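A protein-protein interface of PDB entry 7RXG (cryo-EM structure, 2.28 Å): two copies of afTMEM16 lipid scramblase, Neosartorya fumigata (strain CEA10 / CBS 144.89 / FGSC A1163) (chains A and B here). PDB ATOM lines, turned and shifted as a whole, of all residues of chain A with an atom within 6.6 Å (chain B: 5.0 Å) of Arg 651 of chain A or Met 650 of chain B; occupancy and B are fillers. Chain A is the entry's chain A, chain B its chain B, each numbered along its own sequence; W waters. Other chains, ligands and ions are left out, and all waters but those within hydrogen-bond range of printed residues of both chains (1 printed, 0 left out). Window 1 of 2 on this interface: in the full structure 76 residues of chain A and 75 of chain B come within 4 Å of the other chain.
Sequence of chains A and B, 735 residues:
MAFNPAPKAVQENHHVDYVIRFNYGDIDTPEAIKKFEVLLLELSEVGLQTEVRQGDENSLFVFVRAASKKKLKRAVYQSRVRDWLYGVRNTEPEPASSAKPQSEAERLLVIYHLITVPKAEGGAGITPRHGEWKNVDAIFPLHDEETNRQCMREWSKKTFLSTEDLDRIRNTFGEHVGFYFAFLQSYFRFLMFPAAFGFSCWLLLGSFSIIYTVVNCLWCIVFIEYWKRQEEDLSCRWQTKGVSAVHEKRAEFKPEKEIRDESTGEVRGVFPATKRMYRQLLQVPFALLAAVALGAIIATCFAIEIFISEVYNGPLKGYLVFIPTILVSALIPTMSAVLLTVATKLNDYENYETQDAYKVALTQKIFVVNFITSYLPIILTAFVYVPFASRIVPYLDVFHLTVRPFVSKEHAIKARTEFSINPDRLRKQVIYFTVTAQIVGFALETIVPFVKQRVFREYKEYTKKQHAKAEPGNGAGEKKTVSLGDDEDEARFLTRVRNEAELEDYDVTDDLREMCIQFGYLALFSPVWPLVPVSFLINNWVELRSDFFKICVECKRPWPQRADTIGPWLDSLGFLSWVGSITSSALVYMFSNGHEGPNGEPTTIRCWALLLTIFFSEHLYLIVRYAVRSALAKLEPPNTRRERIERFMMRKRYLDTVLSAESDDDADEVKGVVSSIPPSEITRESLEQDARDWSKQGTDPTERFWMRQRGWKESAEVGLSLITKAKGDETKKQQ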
ATOM      1  N   TRP A  84     -15.320 -35.336 -15.535  1.00  0.00           N
ATOM      2  CA  TRP A  84     -16.434 -34.500 -15.102  1.00  0.00           C
ATOM      3  C   TRP A  84     -17.014 -33.697 -16.256  1.00  0.00           C
ATOM      4  O   TRP A  84     -18.237 -33.585 -16.385  1.00  0.00           O
ATOM      5  CB  TRP A  84     -15.987 -33.571 -13.975  1.00  0.00           C
ATOM      6  CG  TRP A  84     -17.073 -32.671 -13.487  1.00  0.00           C
ATOM      7  CD1 TRP A  84     -18.103 -33.008 -12.672  1.00  0.00           C
ATOM      8  CD2 TRP A  84     -17.237 -31.285 -13.791  1.00  0.00           C
ATOM      9  NE1 TRP A  84     -18.903 -31.921 -12.445  1.00  0.00           N
ATOM     10  CE2 TRP A  84     -18.392 -30.846 -13.119  1.00  0.00           C
ATOM     11  CE3 TRP A  84     -16.520 -30.370 -14.564  1.00  0.00           C
ATOM     12  CZ2 TRP A  84     -18.847 -29.535 -13.197  1.00  0.00           C
ATOM     13  CZ3 TRP A  84     -16.974 -29.071 -14.640  1.00  0.00           C
ATOM     14  CH2 TRP A  84     -18.124 -28.665 -13.961  1.00  0.00           C
ATOM     15  N   LEU A  85     -16.157 -33.131 -17.107  1.00  0.00           N
ATOM     16  CA  LEU A  85     -16.633 -32.334 -18.228  1.00  0.00           C
ATOM     17  C   LEU A  85     -17.456 -33.164 -19.196  1.00  0.00           C
ATOM     18  O   LEU A  85     -18.441 -32.667 -19.749  1.00  0.00           O
ATOM     19  CB  LEU A  85     -15.458 -31.695 -18.967  1.00  0.00           C
ATOM     20  CG  LEU A  85     -14.766 -30.486 -18.341  1.00  0.00           C
ATOM     21  CD1 LEU A  85     -13.669 -29.991 -19.259  1.00  0.00           C
ATOM     22  CD2 LEU A  85     -15.757 -29.377 -18.047  1.00  0.00           C
ATOM     23  N   GLU A  92     -18.085 -32.186  -8.634  1.00  0.00           N
ATOM     24  CA  GLU A  92     -17.043 -31.323  -9.169  1.00  0.00           C
ATOM     25  C   GLU A  92     -15.667 -31.869  -8.793  1.00  0.00           C
ATOM     26  O   GLU A  92     -15.472 -32.343  -7.671  1.00  0.00           O
ATOM     27  CB  GLU A  92     -17.198 -29.897  -8.639  1.00  0.00           C
ATOM     28  CG  GLU A  92     -18.533 -29.240  -8.946  1.00  0.00           C
ATOM     29  CD  GLU A  92     -19.582 -29.522  -7.892  1.00  0.00           C
ATOM     30  OE1 GLU A  92     -19.539 -30.610  -7.286  1.00  0.00           O
ATOM     31  OE2 GLU A  92     -20.451 -28.660  -7.665  1.00  0.00           O
ATOM     32  N   GLU A 646     -27.090 -35.918  -7.378  1.00  0.00           N
ATOM     33  CA  GLU A 646     -25.824 -35.200  -7.388  1.00  0.00           C
ATOM     34  C   GLU A 646     -25.709 -34.288  -8.595  1.00  0.00           C
ATOM     35  O   GLU A 646     -25.111 -33.217  -8.498  1.00  0.00           O
ATOM     36  CB  GLU A 646     -24.654 -36.175  -7.358  1.00  0.00           C
ATOM     37  CG  GLU A 646     -23.307 -35.495  -7.483  1.00  0.00           C
ATOM     38  CD  GLU A 646     -23.109 -34.396  -6.454  1.00  0.00           C
ATOM     39  OE1 GLU A 646     -23.347 -34.651  -5.257  1.00  0.00           O
ATOM     40  OE2 GLU A 646     -22.727 -33.272  -6.845  1.00  0.00           O
ATOM     41  N   ARG A 647     -26.248 -34.698  -9.742  1.00  0.00           N
ATOM     42  CA  ARG A 647     -26.305 -33.781 -10.873  1.00  0.00           C
ATOM     43  C   ARG A 647     -27.135 -32.552 -10.524  1.00  0.00           C
ATOM     44  O   ARG A 647     -26.732 -31.412 -10.810  1.00  0.00           O
ATOM     45  CB  ARG A 647     -26.871 -34.487 -12.102  1.00  0.00           C
ATOM     46  CG  ARG A 647     -26.683 -33.712 -13.382  1.00  0.00           C
ATOM     47  CD  ARG A 647     -26.737 -34.616 -14.602  1.00  0.00           C
ATOM     48  NE  ARG A 647     -28.100 -34.778 -15.104  1.00  0.00           N
ATOM     49  CZ  ARG A 647     -28.775 -33.831 -15.746  1.00  0.00           C
ATOM     50  NH1 ARG A 647     -30.008 -34.062 -16.166  1.00  0.00           N
ATOM     51  NH2 ARG A 647     -28.215 -32.651 -15.967  1.00  0.00           N
ATOM     52  N   PHE A 648     -28.287 -32.767  -9.880  1.00  0.00           N
ATOM     53  CA  PHE A 648     -29.090 -31.637  -9.417  1.00  0.00           C
ATOM     54  C   PHE A 648     -28.293 -30.736  -8.474  1.00  0.00           C
ATOM     55  O   PHE A 648     -28.303 -29.509  -8.613  1.00  0.00           O
ATOM     56  CB  PHE A 648     -30.363 -32.137  -8.734  1.00  0.00           C
ATOM     57  CG  PHE A 648     -31.183 -31.045  -8.105  1.00  0.00           C
ATOM     58  CD1 PHE A 648     -32.081 -30.317  -8.860  1.00  0.00           C
ATOM     59  CD2 PHE A 648     -31.059 -30.750  -6.759  1.00  0.00           C
ATOM     60  CE1 PHE A 648     -32.833 -29.315  -8.290  1.00  0.00           C
ATOM     61  CE2 PHE A 648     -31.804 -29.743  -6.186  1.00  0.00           C
ATOM     62  CZ  PHE A 648     -32.691 -29.027  -6.953  1.00  0.00           C
ATOM     63  N   MET A 649     -27.598 -31.333  -7.504  1.00  0.00           N
ATOM     64  CA  MET A 649     -26.861 -30.558  -6.513  1.00  0.00           C
ATOM     65  C   MET A 649     -25.688 -29.806  -7.131  1.00  0.00           C
ATOM     66  O   MET A 649     -25.386 -28.687  -6.712  1.00  0.00           O
ATOM     67  CB  MET A 649     -26.368 -31.469  -5.391  1.00  0.00           C
ATOM     68  CG  MET A 649     -27.466 -32.006  -4.495  1.00  0.00           C
ATOM     69  SD  MET A 649     -28.482 -30.700  -3.787  1.00  0.00           S
ATOM     70  CE  MET A 649     -27.221 -29.659  -3.055  1.00  0.00           C
ATOM     71  N   MET A 650     -25.014 -30.399  -8.114  1.00  0.00           N
ATOM     72  CA  MET A 650     -23.935 -29.696  -8.794  1.00  0.00           C
ATOM     73  C   MET A 650     -24.464 -28.485  -9.545  1.00  0.00           C
ATOM     74  O   MET A 650     -23.866 -27.400  -9.495  1.00  0.00           O
ATOM     75  CB  MET A 650     -23.203 -30.642  -9.746  1.00  0.00           C
ATOM     76  CG  MET A 650     -22.045 -30.000 -10.491  1.00  0.00           C
ATOM     77  SD  MET A 650     -22.500 -29.336 -12.103  1.00  0.00           S
ATOM     78  CE  MET A 650     -23.172 -30.792 -12.885  1.00  0.00           C
ATOM     79  N   ARG A 651     -25.583 -28.646 -10.258  1.00  0.00           N
ATOM     80  CA  ARG A 651     -26.152 -27.489 -10.938  1.00  0.00           C
ATOM     81  C   ARG A 651     -26.620 -26.437  -9.942  1.00  0.00           C
ATOM     82  O   ARG A 651     -26.524 -25.239 -10.218  1.00  0.00           O
ATOM     83  CB  ARG A 651     -27.289 -27.920 -11.860  1.00  0.00           C
ATOM     84  CG  ARG A 651     -26.792 -28.533 -13.147  1.00  0.00           C
ATOM     85  CD  ARG A 651     -27.865 -28.636 -14.195  1.00  0.00           C
ATOM     86  NE  ARG A 651     -27.361 -29.311 -15.382  1.00  0.00           N
ATOM     87  CZ  ARG A 651     -27.932 -29.262 -16.577  1.00  0.00           C
ATOM     88  NH1 ARG A 651     -27.391 -29.909 -17.595  1.00  0.00           N
ATOM     89  NH2 ARG A 651     -29.039 -28.567 -16.755  1.00  0.00           N
ATOM     90  N   LYS A 652     -27.091 -26.863  -8.772  1.00  0.00           N
ATOM     91  CA  LYS A 652     -27.490 -25.910  -7.743  1.00  0.00           C
ATOM     92  C   LYS A 652     -26.289 -25.147  -7.194  1.00  0.00           C
ATOM     93  O   LYS A 652     -26.382 -23.944  -6.939  1.00  0.00           O
ATOM     94  CB  LYS A 652     -28.235 -26.637  -6.625  1.00  0.00           C
ATOM     95  CG  LYS A 652     -28.888 -25.729  -5.609  1.00  0.00           C
ATOM     96  CD  LYS A 652     -29.804 -24.723  -6.274  1.00  0.00           C
ATOM     97  CE  LYS A 652     -30.853 -24.205  -5.307  1.00  0.00           C
ATOM     98  NZ  LYS A 652     -30.240 -23.573  -4.108  1.00  0.00           N
ATOM     99  N   ARG A 653     -25.154 -25.825  -7.005  1.00  0.00           N
ATOM    100  CA  ARG A 653     -23.937 -25.133  -6.583  1.00  0.00           C
ATOM    101  C   ARG A 653     -23.488 -24.121  -7.627  1.00  0.00           C
ATOM    102  O   ARG A 653     -23.075 -23.007  -7.285  1.00  0.00           O
ATOM    103  CB  ARG A 653     -22.811 -26.130  -6.317  1.00  0.00           C
ATOM    104  CG  ARG A 653     -22.920 -26.883  -5.021  1.00  0.00           C
ATOM    105  CD  ARG A 653     -21.878 -27.980  -4.942  1.00  0.00           C
ATOM    106  NE  ARG A 653     -22.432 -29.174  -4.321  1.00  0.00           N
ATOM    107  CZ  ARG A 653     -22.497 -30.364  -4.903  1.00  0.00           C
ATOM    108  NH1 ARG A 653     -22.020 -30.540  -6.123  1.00  0.00           N
ATOM    109  NH2 ARG A 653     -23.033 -31.382  -4.250  1.00  0.00           N
ATOM    110  N   TYR A 654     -23.538 -24.506  -8.902  1.00  0.00           N
ATOM    111  CA  TYR A 654     -23.216 -23.568  -9.973  1.00  0.00           C
ATOM    112  C   TYR A 654     -24.134 -22.353  -9.924  1.00  0.00           C
ATOM    113  O   TYR A 654     -23.667 -21.211  -9.995  1.00  0.00           O
ATOM    114  CB  TYR A 654     -23.311 -24.284 -11.320  1.00  0.00           C
ATOM    115  CG  TYR A 654     -22.911 -23.491 -12.545  1.00  0.00           C
ATOM    116  CD1 TYR A 654     -22.124 -22.353 -12.454  1.00  0.00           C
ATOM    117  CD2 TYR A 654     -23.310 -23.903 -13.802  1.00  0.00           C
ATOM    118  CE1 TYR A 654     -21.765 -21.648 -13.576  1.00  0.00           C
ATOM    119  CE2 TYR A 654     -22.956 -23.206 -14.925  1.00  0.00           C
ATOM    120  CZ  TYR A 654     -22.185 -22.080 -14.810  1.00  0.00           C
ATOM    121  OH  TYR A 654     -21.833 -21.389 -15.940  1.00  0.00           O
ATOM    122  N   LEU A 655     -25.442 -22.580  -9.784  1.00  0.00           N
ATOM    123  CA  LEU A 655     -26.394 -21.477  -9.740  1.00  0.00           C
ATOM    124  C   LEU A 655     -26.201 -20.601  -8.508  1.00  0.00           C
ATOM    125  O   LEU A 655     -26.470 -19.398  -8.556  1.00  0.00           O
ATOM    126  CB  LEU A 655     -27.822 -22.018  -9.777  1.00  0.00           C
ATOM    127  CG  LEU A 655     -28.937 -20.977  -9.702  1.00  0.00           C
ATOM    128  CD1 LEU A 655     -29.309 -20.495 -11.086  1.00  0.00           C
ATOM    129  CD2 LEU A 655     -30.147 -21.541  -8.983  1.00  0.00           C
ATOM    130  N   ASP A 656     -25.763 -21.182  -7.397  1.00  0.00           N
ATOM    131  CA  ASP A 656     -25.590 -20.417  -6.173  1.00  0.00           C
ATOM    132  C   ASP A 656     -24.287 -19.633  -6.148  1.00  0.00           C
ATOM    133  O   ASP A 656     -24.236 -18.571  -5.520  1.00  0.00           O
ATOM    134  CB  ASP A 656     -25.663 -21.348  -4.961  1.00  0.00           C
ATOM    135  CG  ASP A 656     -27.083 -21.775  -4.638  1.00  0.00           C
ATOM    136  OD1 ASP A 656     -28.017 -21.344  -5.347  1.00  0.00           O
ATOM    137  OD2 ASP A 656     -27.271 -22.542  -3.672  1.00  0.00           O
ATOM    138  N   LEU A 659     -24.197 -16.987 -11.517  1.00  0.00           N
ATOM    139  CA  LEU A 659     -25.610 -16.847 -11.862  1.00  0.00           C
ATOM    140  C   LEU A 659     -26.448 -16.357 -10.681  1.00  0.00           C
ATOM    141  O   LEU A 659     -27.680 -16.411 -10.725  1.00  0.00           O
ATOM    142  CB  LEU A 659     -26.189 -18.163 -12.405  1.00  0.00           C
ATOM    143  CG  LEU A 659     -25.308 -19.082 -13.267  1.00  0.00           C
ATOM    144  CD1 LEU A 659     -26.076 -20.331 -13.677  1.00  0.00           C
ATOM    145  CD2 LEU A 659     -24.761 -18.364 -14.488  1.00  0.00           C
ATOM    146  N   TRP B  84     -33.702 -25.885 -15.706  1.00  0.00           N
ATOM    147  CA  TRP B  84     -32.263 -26.086 -15.836  1.00  0.00           C
ATOM    148  C   TRP B  84     -31.713 -26.948 -14.709  1.00  0.00           C
ATOM    149  O   TRP B  84     -30.885 -27.832 -14.948  1.00  0.00           O
ATOM    150  CB  TRP B  84     -31.546 -24.738 -15.877  1.00  0.00           C
ATOM    151  CG  TRP B  84     -30.063 -24.862 -15.994  1.00  0.00           C
ATOM    152  CD1 TRP B  84     -29.357 -25.164 -17.112  1.00  0.00           C
ATOM    153  CD2 TRP B  84     -29.104 -24.693 -14.947  1.00  0.00           C
ATOM    154  NE1 TRP B  84     -28.017 -25.194 -16.835  1.00  0.00           N
ATOM    155  CE2 TRP B  84     -27.833 -24.906 -15.510  1.00  0.00           C
ATOM    156  CE3 TRP B  84     -29.195 -24.382 -13.590  1.00  0.00           C
ATOM    157  CZ2 TRP B  84     -26.664 -24.817 -14.764  1.00  0.00           C
ATOM    158  CZ3 TRP B  84     -28.034 -24.295 -12.853  1.00  0.00           C
ATOM    159  CH2 TRP B  84     -26.786 -24.512 -13.440  1.00  0.00           C
ATOM    160  N   LEU B  85     -32.160 -26.709 -13.475  1.00  0.00           N
ATOM    161  CA  LEU B  85     -31.672 -27.481 -12.341  1.00  0.00           C
ATOM    162  C   LEU B  85     -32.024 -28.950 -12.471  1.00  0.00           C
ATOM    163  O   LEU B  85     -31.226 -29.810 -12.090  1.00  0.00           O
ATOM    164  CB  LEU B  85     -32.239 -26.927 -11.035  1.00  0.00           C
ATOM    165  CG  LEU B  85     -31.652 -25.636 -10.467  1.00  0.00           C
ATOM    166  CD1 LEU B  85     -32.326 -25.300  -9.155  1.00  0.00           C
ATOM    167  CD2 LEU B  85     -30.152 -25.747 -10.286  1.00  0.00           C
ATOM    168  N   GLY B  87     -32.246 -30.533 -15.227  1.00  0.00           N
ATOM    169  CA  GLY B  87     -31.646 -31.062 -16.430  1.00  0.00           C
ATOM    170  C   GLY B  87     -32.511 -31.022 -17.669  1.00  0.00           C
ATOM    171  O   GLY B  87     -32.108 -31.577 -18.696  1.00  0.00           O
ATOM    172  N   ARG B  89     -33.146 -28.425 -19.484  1.00  0.00           N
ATOM    173  CA  ARG B  89     -32.354 -27.620 -20.403  1.00  0.00           C
ATOM    174  C   ARG B  89     -30.908 -27.643 -19.935  1.00  0.00           C
ATOM    175  O   ARG B  89     -30.639 -27.910 -18.761  1.00  0.00           O
ATOM    176  CB  ARG B  89     -32.871 -26.182 -20.475  1.00  0.00           C
ATOM    177  CG  ARG B  89     -33.295 -25.613 -19.139  1.00  0.00           C
ATOM    178  CD  ARG B  89     -33.979 -24.268 -19.295  1.00  0.00           C
ATOM    179  NE  ARG B  89     -33.025 -23.205 -19.589  1.00  0.00           N
ATOM    180  CZ  ARG B  89     -33.343 -22.054 -20.172  1.00  0.00           C
ATOM    181  NH1 ARG B  89     -34.598 -21.811 -20.528  1.00  0.00           N
ATOM    182  NH2 ARG B  89     -32.405 -21.147 -20.401  1.00  0.00           N
ATOM    183  N   ASN B  90     -29.980 -27.360 -20.848  1.00  0.00           N
ATOM    184  CA  ASN B  90     -28.568 -27.387 -20.484  1.00  0.00           C
ATOM    185  C   ASN B  90     -27.972 -25.988 -20.454  1.00  0.00           C
ATOM    186  O   ASN B  90     -27.054 -25.719 -19.674  1.00  0.00           O
ATOM    187  CB  ASN B  90     -27.796 -28.285 -21.445  1.00  0.00           C
ATOM    188  CG  ASN B  90     -28.049 -29.755 -21.193  1.00  0.00           C
ATOM    189  OD1 ASN B  90     -28.409 -30.150 -20.088  1.00  0.00           O
ATOM    190  ND2 ASN B  90     -27.867 -30.571 -22.219  1.00  0.00           N
ATOM    191  N   GLU B  92     -27.481 -22.283 -19.384  1.00  0.00           N
ATOM    192  CA  GLU B  92     -27.740 -21.613 -18.119  1.00  0.00           C
ATOM    193  C   GLU B  92     -28.885 -20.615 -18.280  1.00  0.00           C
ATOM    194  O   GLU B  92     -28.968 -19.924 -19.299  1.00  0.00           O
ATOM    195  CB  GLU B  92     -26.487 -20.890 -17.623  1.00  0.00           C
ATOM    196  CG  GLU B  92     -25.270 -21.778 -17.425  1.00  0.00           C
ATOM    197  CD  GLU B  92     -24.438 -21.921 -18.680  1.00  0.00           C
ATOM    198  OE1 GLU B  92     -25.012 -21.876 -19.785  1.00  0.00           O
ATOM    199  OE2 GLU B  92     -23.207 -22.076 -18.569  1.00  0.00           O
ATOM    200  N   GLU B 646     -23.785 -28.945 -25.591  1.00  0.00           N
ATOM    201  CA  GLU B 646     -24.116 -27.835 -24.710  1.00  0.00           C
ATOM    202  C   GLU B 646     -23.962 -28.216 -23.250  1.00  0.00           C
ATOM    203  O   GLU B 646     -23.583 -27.375 -22.435  1.00  0.00           O
ATOM    204  CB  GLU B 646     -25.536 -27.347 -24.974  1.00  0.00           C
ATOM    205  CG  GLU B 646     -25.985 -26.268 -24.011  1.00  0.00           C
ATOM    206  CD  GLU B 646     -25.021 -25.096 -23.956  1.00  0.00           C
ATOM    207  OE1 GLU B 646     -24.649 -24.581 -25.029  1.00  0.00           O
ATOM    208  OE2 GLU B 646     -24.626 -24.698 -22.839  1.00  0.00           O
ATOM    209  N   ARG B 647     -24.269 -29.462 -22.893  1.00  0.00           N
ATOM    210  CA  ARG B 647     -23.974 -29.910 -21.538  1.00  0.00           C
ATOM    211  C   ARG B 647     -22.478 -29.835 -21.263  1.00  0.00           C
ATOM    212  O   ARG B 647     -22.050 -29.349 -20.203  1.00  0.00           O
ATOM    213  CB  ARG B 647     -24.495 -31.329 -21.322  1.00  0.00           C
ATOM    214  CG  ARG B 647     -24.505 -31.753 -19.874  1.00  0.00           C
ATOM    215  CD  ARG B 647     -25.490 -32.882 -19.625  1.00  0.00           C
ATOM    216  NE  ARG B 647     -24.882 -34.195 -19.826  1.00  0.00           N
ATOM    217  CZ  ARG B 647     -24.004 -34.745 -18.993  1.00  0.00           C
ATOM    218  NH1 ARG B 647     -23.500 -35.941 -19.253  1.00  0.00           N
ATOM    219  NH2 ARG B 647     -23.631 -34.096 -17.901  1.00  0.00           N
ATOM    220  N   PHE B 648     -21.667 -30.287 -22.225  1.00  0.00           N
ATOM    221  CA  PHE B 648     -20.218 -30.155 -22.085  1.00  0.00           C
ATOM    222  C   PHE B 648     -19.807 -28.694 -21.902  1.00  0.00           C
ATOM    223  O   PHE B 648     -19.005 -28.368 -21.022  1.00  0.00           O
ATOM    224  CB  PHE B 648     -19.510 -30.763 -23.297  1.00  0.00           C
ATOM    225  CG  PHE B 648     -18.022 -30.549 -23.301  1.00  0.00           C
ATOM    226  CD1 PHE B 648     -17.188 -31.399 -22.603  1.00  0.00           C
ATOM    227  CD2 PHE B 648     -17.459 -29.499 -24.005  1.00  0.00           C
ATOM    228  CE1 PHE B 648     -15.825 -31.206 -22.602  1.00  0.00           C
ATOM    229  CE2 PHE B 648     -16.097 -29.299 -24.002  1.00  0.00           C
ATOM    230  CZ  PHE B 648     -15.280 -30.154 -23.300  1.00  0.00           C
ATOM    231  N   MET B 649     -20.350 -27.801 -22.731  1.00  0.00           N
ATOM    232  CA  MET B 649     -19.971 -26.392 -22.680  1.00  0.00           C
ATOM    233  C   MET B 649     -20.419 -25.724 -21.387  1.00  0.00           C
ATOM    234  O   MET B 649     -19.709 -24.864 -20.862  1.00  0.00           O
ATOM    235  CB  MET B 649     -20.548 -25.648 -23.883  1.00  0.00           C
ATOM    236  CG  MET B 649     -19.909 -26.013 -25.208  1.00  0.00           C
ATOM    237  SD  MET B 649     -18.122 -25.809 -25.195  1.00  0.00           S
ATOM    238  CE  MET B 649     -17.986 -24.117 -24.624  1.00  0.00           C
ATOM    239  N   MET B 650     -21.586 -26.095 -20.864  1.00  0.00           N
ATOM    240  CA  MET B 650     -22.027 -25.548 -19.588  1.00  0.00           C
ATOM    241  C   MET B 650     -21.099 -25.976 -18.463  1.00  0.00           C
ATOM    242  O   MET B 650     -20.726 -25.161 -17.608  1.00  0.00           O
ATOM    243  CB  MET B 650     -23.463 -25.980 -19.294  1.00  0.00           C
ATOM    244  CG  MET B 650     -24.020 -25.440 -17.988  1.00  0.00           C
ATOM    245  SD  MET B 650     -23.797 -26.557 -16.591  1.00  0.00           S
ATOM    246  CE  MET B 650     -24.616 -28.020 -17.201  1.00  0.00           C
ATOM    247  N   ARG B 651     -20.717 -27.257 -18.438  1.00  0.00           N
ATOM    248  CA  ARG B 651     -19.776 -27.686 -17.409  1.00  0.00           C
ATOM    249  C   ARG B 651     -18.424 -27.008 -17.580  1.00  0.00           C
ATOM    250  O   ARG B 651     -17.754 -26.708 -16.589  1.00  0.00           O
ATOM    251  CB  ARG B 651     -19.636 -29.205 -17.417  1.00  0.00           C
ATOM    252  CG  ARG B 651     -20.802 -29.898 -16.754  1.00  0.00           C
ATOM    253  CD  ARG B 651     -20.520 -31.343 -16.443  1.00  0.00           C
ATOM    254  NE  ARG B 651     -21.701 -31.988 -15.887  1.00  0.00           N
ATOM    255  CZ  ARG B 651     -21.688 -33.129 -15.212  1.00  0.00           C
ATOM    256  NH1 ARG B 651     -22.818 -33.631 -14.743  1.00  0.00           N
ATOM    257  NH2 ARG B 651     -20.550 -33.766 -15.005  1.00  0.00           N
ATOM    258  N   LYS B 652     -18.026 -26.729 -18.820  1.00  0.00           N
ATOM    259  CA  LYS B 652     -16.777 -26.016 -19.053  1.00  0.00           C
ATOM    260  C   LYS B 652     -16.852 -24.577 -18.552  1.00  0.00           C
ATOM    261  O   LYS B 652     -15.882 -24.065 -17.989  1.00  0.00           O
ATOM    262  CB  LYS B 652     -16.425 -26.062 -20.539  1.00  0.00           C
ATOM    263  CG  LYS B 652     -15.044 -25.548 -20.876  1.00  0.00           C
ATOM    264  CD  LYS B 652     -13.978 -26.258 -20.069  1.00  0.00           C
ATOM    265  CE  LYS B 652     -12.624 -26.180 -20.751  1.00  0.00           C
ATOM    266  NZ  LYS B 652     -12.194 -24.775 -20.978  1.00  0.00           N
ATOM    267  N   ARG B 653     -17.993 -23.910 -18.748  1.00  0.00           N
ATOM    268  CA  ARG B 653     -18.169 -22.565 -18.199  1.00  0.00           C
ATOM    269  C   ARG B 653     -18.109 -22.579 -16.679  1.00  0.00           C
ATOM    270  O   ARG B 653     -17.499 -21.694 -16.067  1.00  0.00           O
ATOM    271  CB  ARG B 653     -19.496 -21.964 -18.655  1.00  0.00           C
ATOM    272  CG  ARG B 653     -19.517 -21.468 -20.074  1.00  0.00           C
ATOM    273  CD  ARG B 653     -20.921 -21.079 -20.491  1.00  0.00           C
ATOM    274  NE  ARG B 653     -21.176 -21.472 -21.868  1.00  0.00           N
ATOM    275  CZ  ARG B 653     -22.142 -22.297 -22.248  1.00  0.00           C
ATOM    276  NH1 ARG B 653     -22.973 -22.812 -21.358  1.00  0.00           N
ATOM    277  NH2 ARG B 653     -22.279 -22.598 -23.530  1.00  0.00           N
ATOM    278  N   TYR B 654     -18.759 -23.561 -16.056  1.00  0.00           N
ATOM    279  CA  TYR B 654     -18.675 -23.704 -14.607  1.00  0.00           C
ATOM    280  C   TYR B 654     -17.228 -23.886 -14.161  1.00  0.00           C
ATOM    281  O   TYR B 654     -16.771 -23.218 -13.228  1.00  0.00           O
ATOM    282  CB  TYR B 654     -19.546 -24.878 -14.162  1.00  0.00           C
ATOM    283  CG  TYR B 654     -19.663 -25.115 -12.672  1.00  0.00           C
ATOM    284  CD1 TYR B 654     -19.363 -24.125 -11.747  1.00  0.00           C
ATOM    285  CD2 TYR B 654     -20.099 -26.337 -12.193  1.00  0.00           C
ATOM    286  CE1 TYR B 654     -19.481 -24.355 -10.399  1.00  0.00           C
ATOM    287  CE2 TYR B 654     -20.219 -26.573 -10.850  1.00  0.00           C
ATOM    288  CZ  TYR B 654     -19.909 -25.582  -9.956  1.00  0.00           C
ATOM    289  OH  TYR B 654     -20.035 -25.828  -8.613  1.00  0.00           O
HETATM  290  O   HOH W   1     -29.192 -32.477 -19.134  1.00  0.00           O
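Hydrophobic or aromatic side chains of chain B that line the printed part of chain A: Trp 84, Leu 85, Phe 648, Met 650 and Tyr 654. Hydrophobic or aromatic side chains of chain A that line the printed part of chain B: Trp 84, Leu 85, Phe 648, Met 650, Tyr 654 and Leu 655. Among the printed residues, 24 pairs touch across the chains.
The guanidinium group (NH1) of Arg 653 of chain B lies within salt-bridge range of the side-chain carboxylate (OE2) of Glu 646 of chain B. NH1 of Arg 653 of chain A is in salt-bridge range of OE1 of Glu 92 of chain A (2.7 Å). NZ of Lys 652 of chain A lies within salt-bridge range of OD2 of Asp 656 of chain A, at 3.2 Å.
The backbone carbonyl oxygen of Trp 84 of chain B sits at hydrogen-bond distance from the guanidinium group of Arg 651 of chain A (2.7 Å). The backbone carbonyl oxygen (O) of Arg 89 of chain B is in hydrogen-bond range of the guanidinium group (NH2) of Arg 651 of chain A, at 2.6 Å. The side-chain amide oxygen (OD1) of Asn 90 of chain B is in hydrogen-bond range of the guanidinium group (NH1) of Arg 651 of chain A. The side-chain carboxylate (OE2) of Glu 92 of chain B is in hydrogen-bond range of the side-chain hydroxyl (OH) of Tyr 654 of chain A. The guanidinium group of Arg 651 of chain B lies within hydrogen-bond range of the backbone carbonyl oxygen of Trp 84 of chain A (2.7 Å). The side-chain hydroxyl (OH) of Tyr 654 of chain B sits at hydrogen-bond distance from the side-chain carboxylate (OE2) of Glu 92 of chain A (3.0 Å).
Arg 651 of chain A touches just these residues of chain B: Trp 84, Leu 85, Gly 87, Arg 89, Asn 90 and Met 650. Printed residues of chain A within 4 Å of Leu 85 of chain B: Phe 648, Arg 651 and Lys 652. Glu 646 of chain B touches none of the printed residues of chain A. Printed residues of chain A within 4 Å of Met 650 of chain B: Arg 651 and Tyr 654. Printed residues of chain A within 4 Å of Tyr 654 of chain B: Trp 84, Glu 92, Met 650, Arg 653 and Tyr 654. The nearest residue of chain B that does not touch Arg 651 of chain A is Arg 647 of chain B (4.1 Å). The nearest residue of chain A that does not touch Met 650 of chain B is Met 650 of chain A (5.3 Å). The nearest printed residue of chain B that does not touch Leu 85 of chain A is Arg 647 of chain B (4.9 Å).
CD1 of Phe 648 of chain B touches O of Leu 85 of chain A (3.4 Å). Leu 85 of chain A touches Lys 652 of chain B (CD2 to N, 3.6 Å). NH1 of Arg 647 of chain A touches CA of Gly 87 of chain B, 3.4 Å away. Met 650 of chain A touches Arg 651 of chain B (CE to NH1, 3.4 Å). Gly 87 of chain B touches Arg 651 of chain A (CA to NH2, 3.6 Å).
Trp 84 of chain A touches Tyr 654 of chain B, and with the chains exchanged Tyr 654 of chain A touches Trp 84 of chain B. Leu 85 of chain A touches Arg 651 of chain B, and with the chains exchanged Arg 651 of chain A touches Leu 85 of chain B.
Water W1 lies within hydrogen-bond range of OD1 of Asn 90 of chain B, O of Gly 87 of chain B, NH2 of Arg 647 of chain A and NH1 of Arg 651 of chain A.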
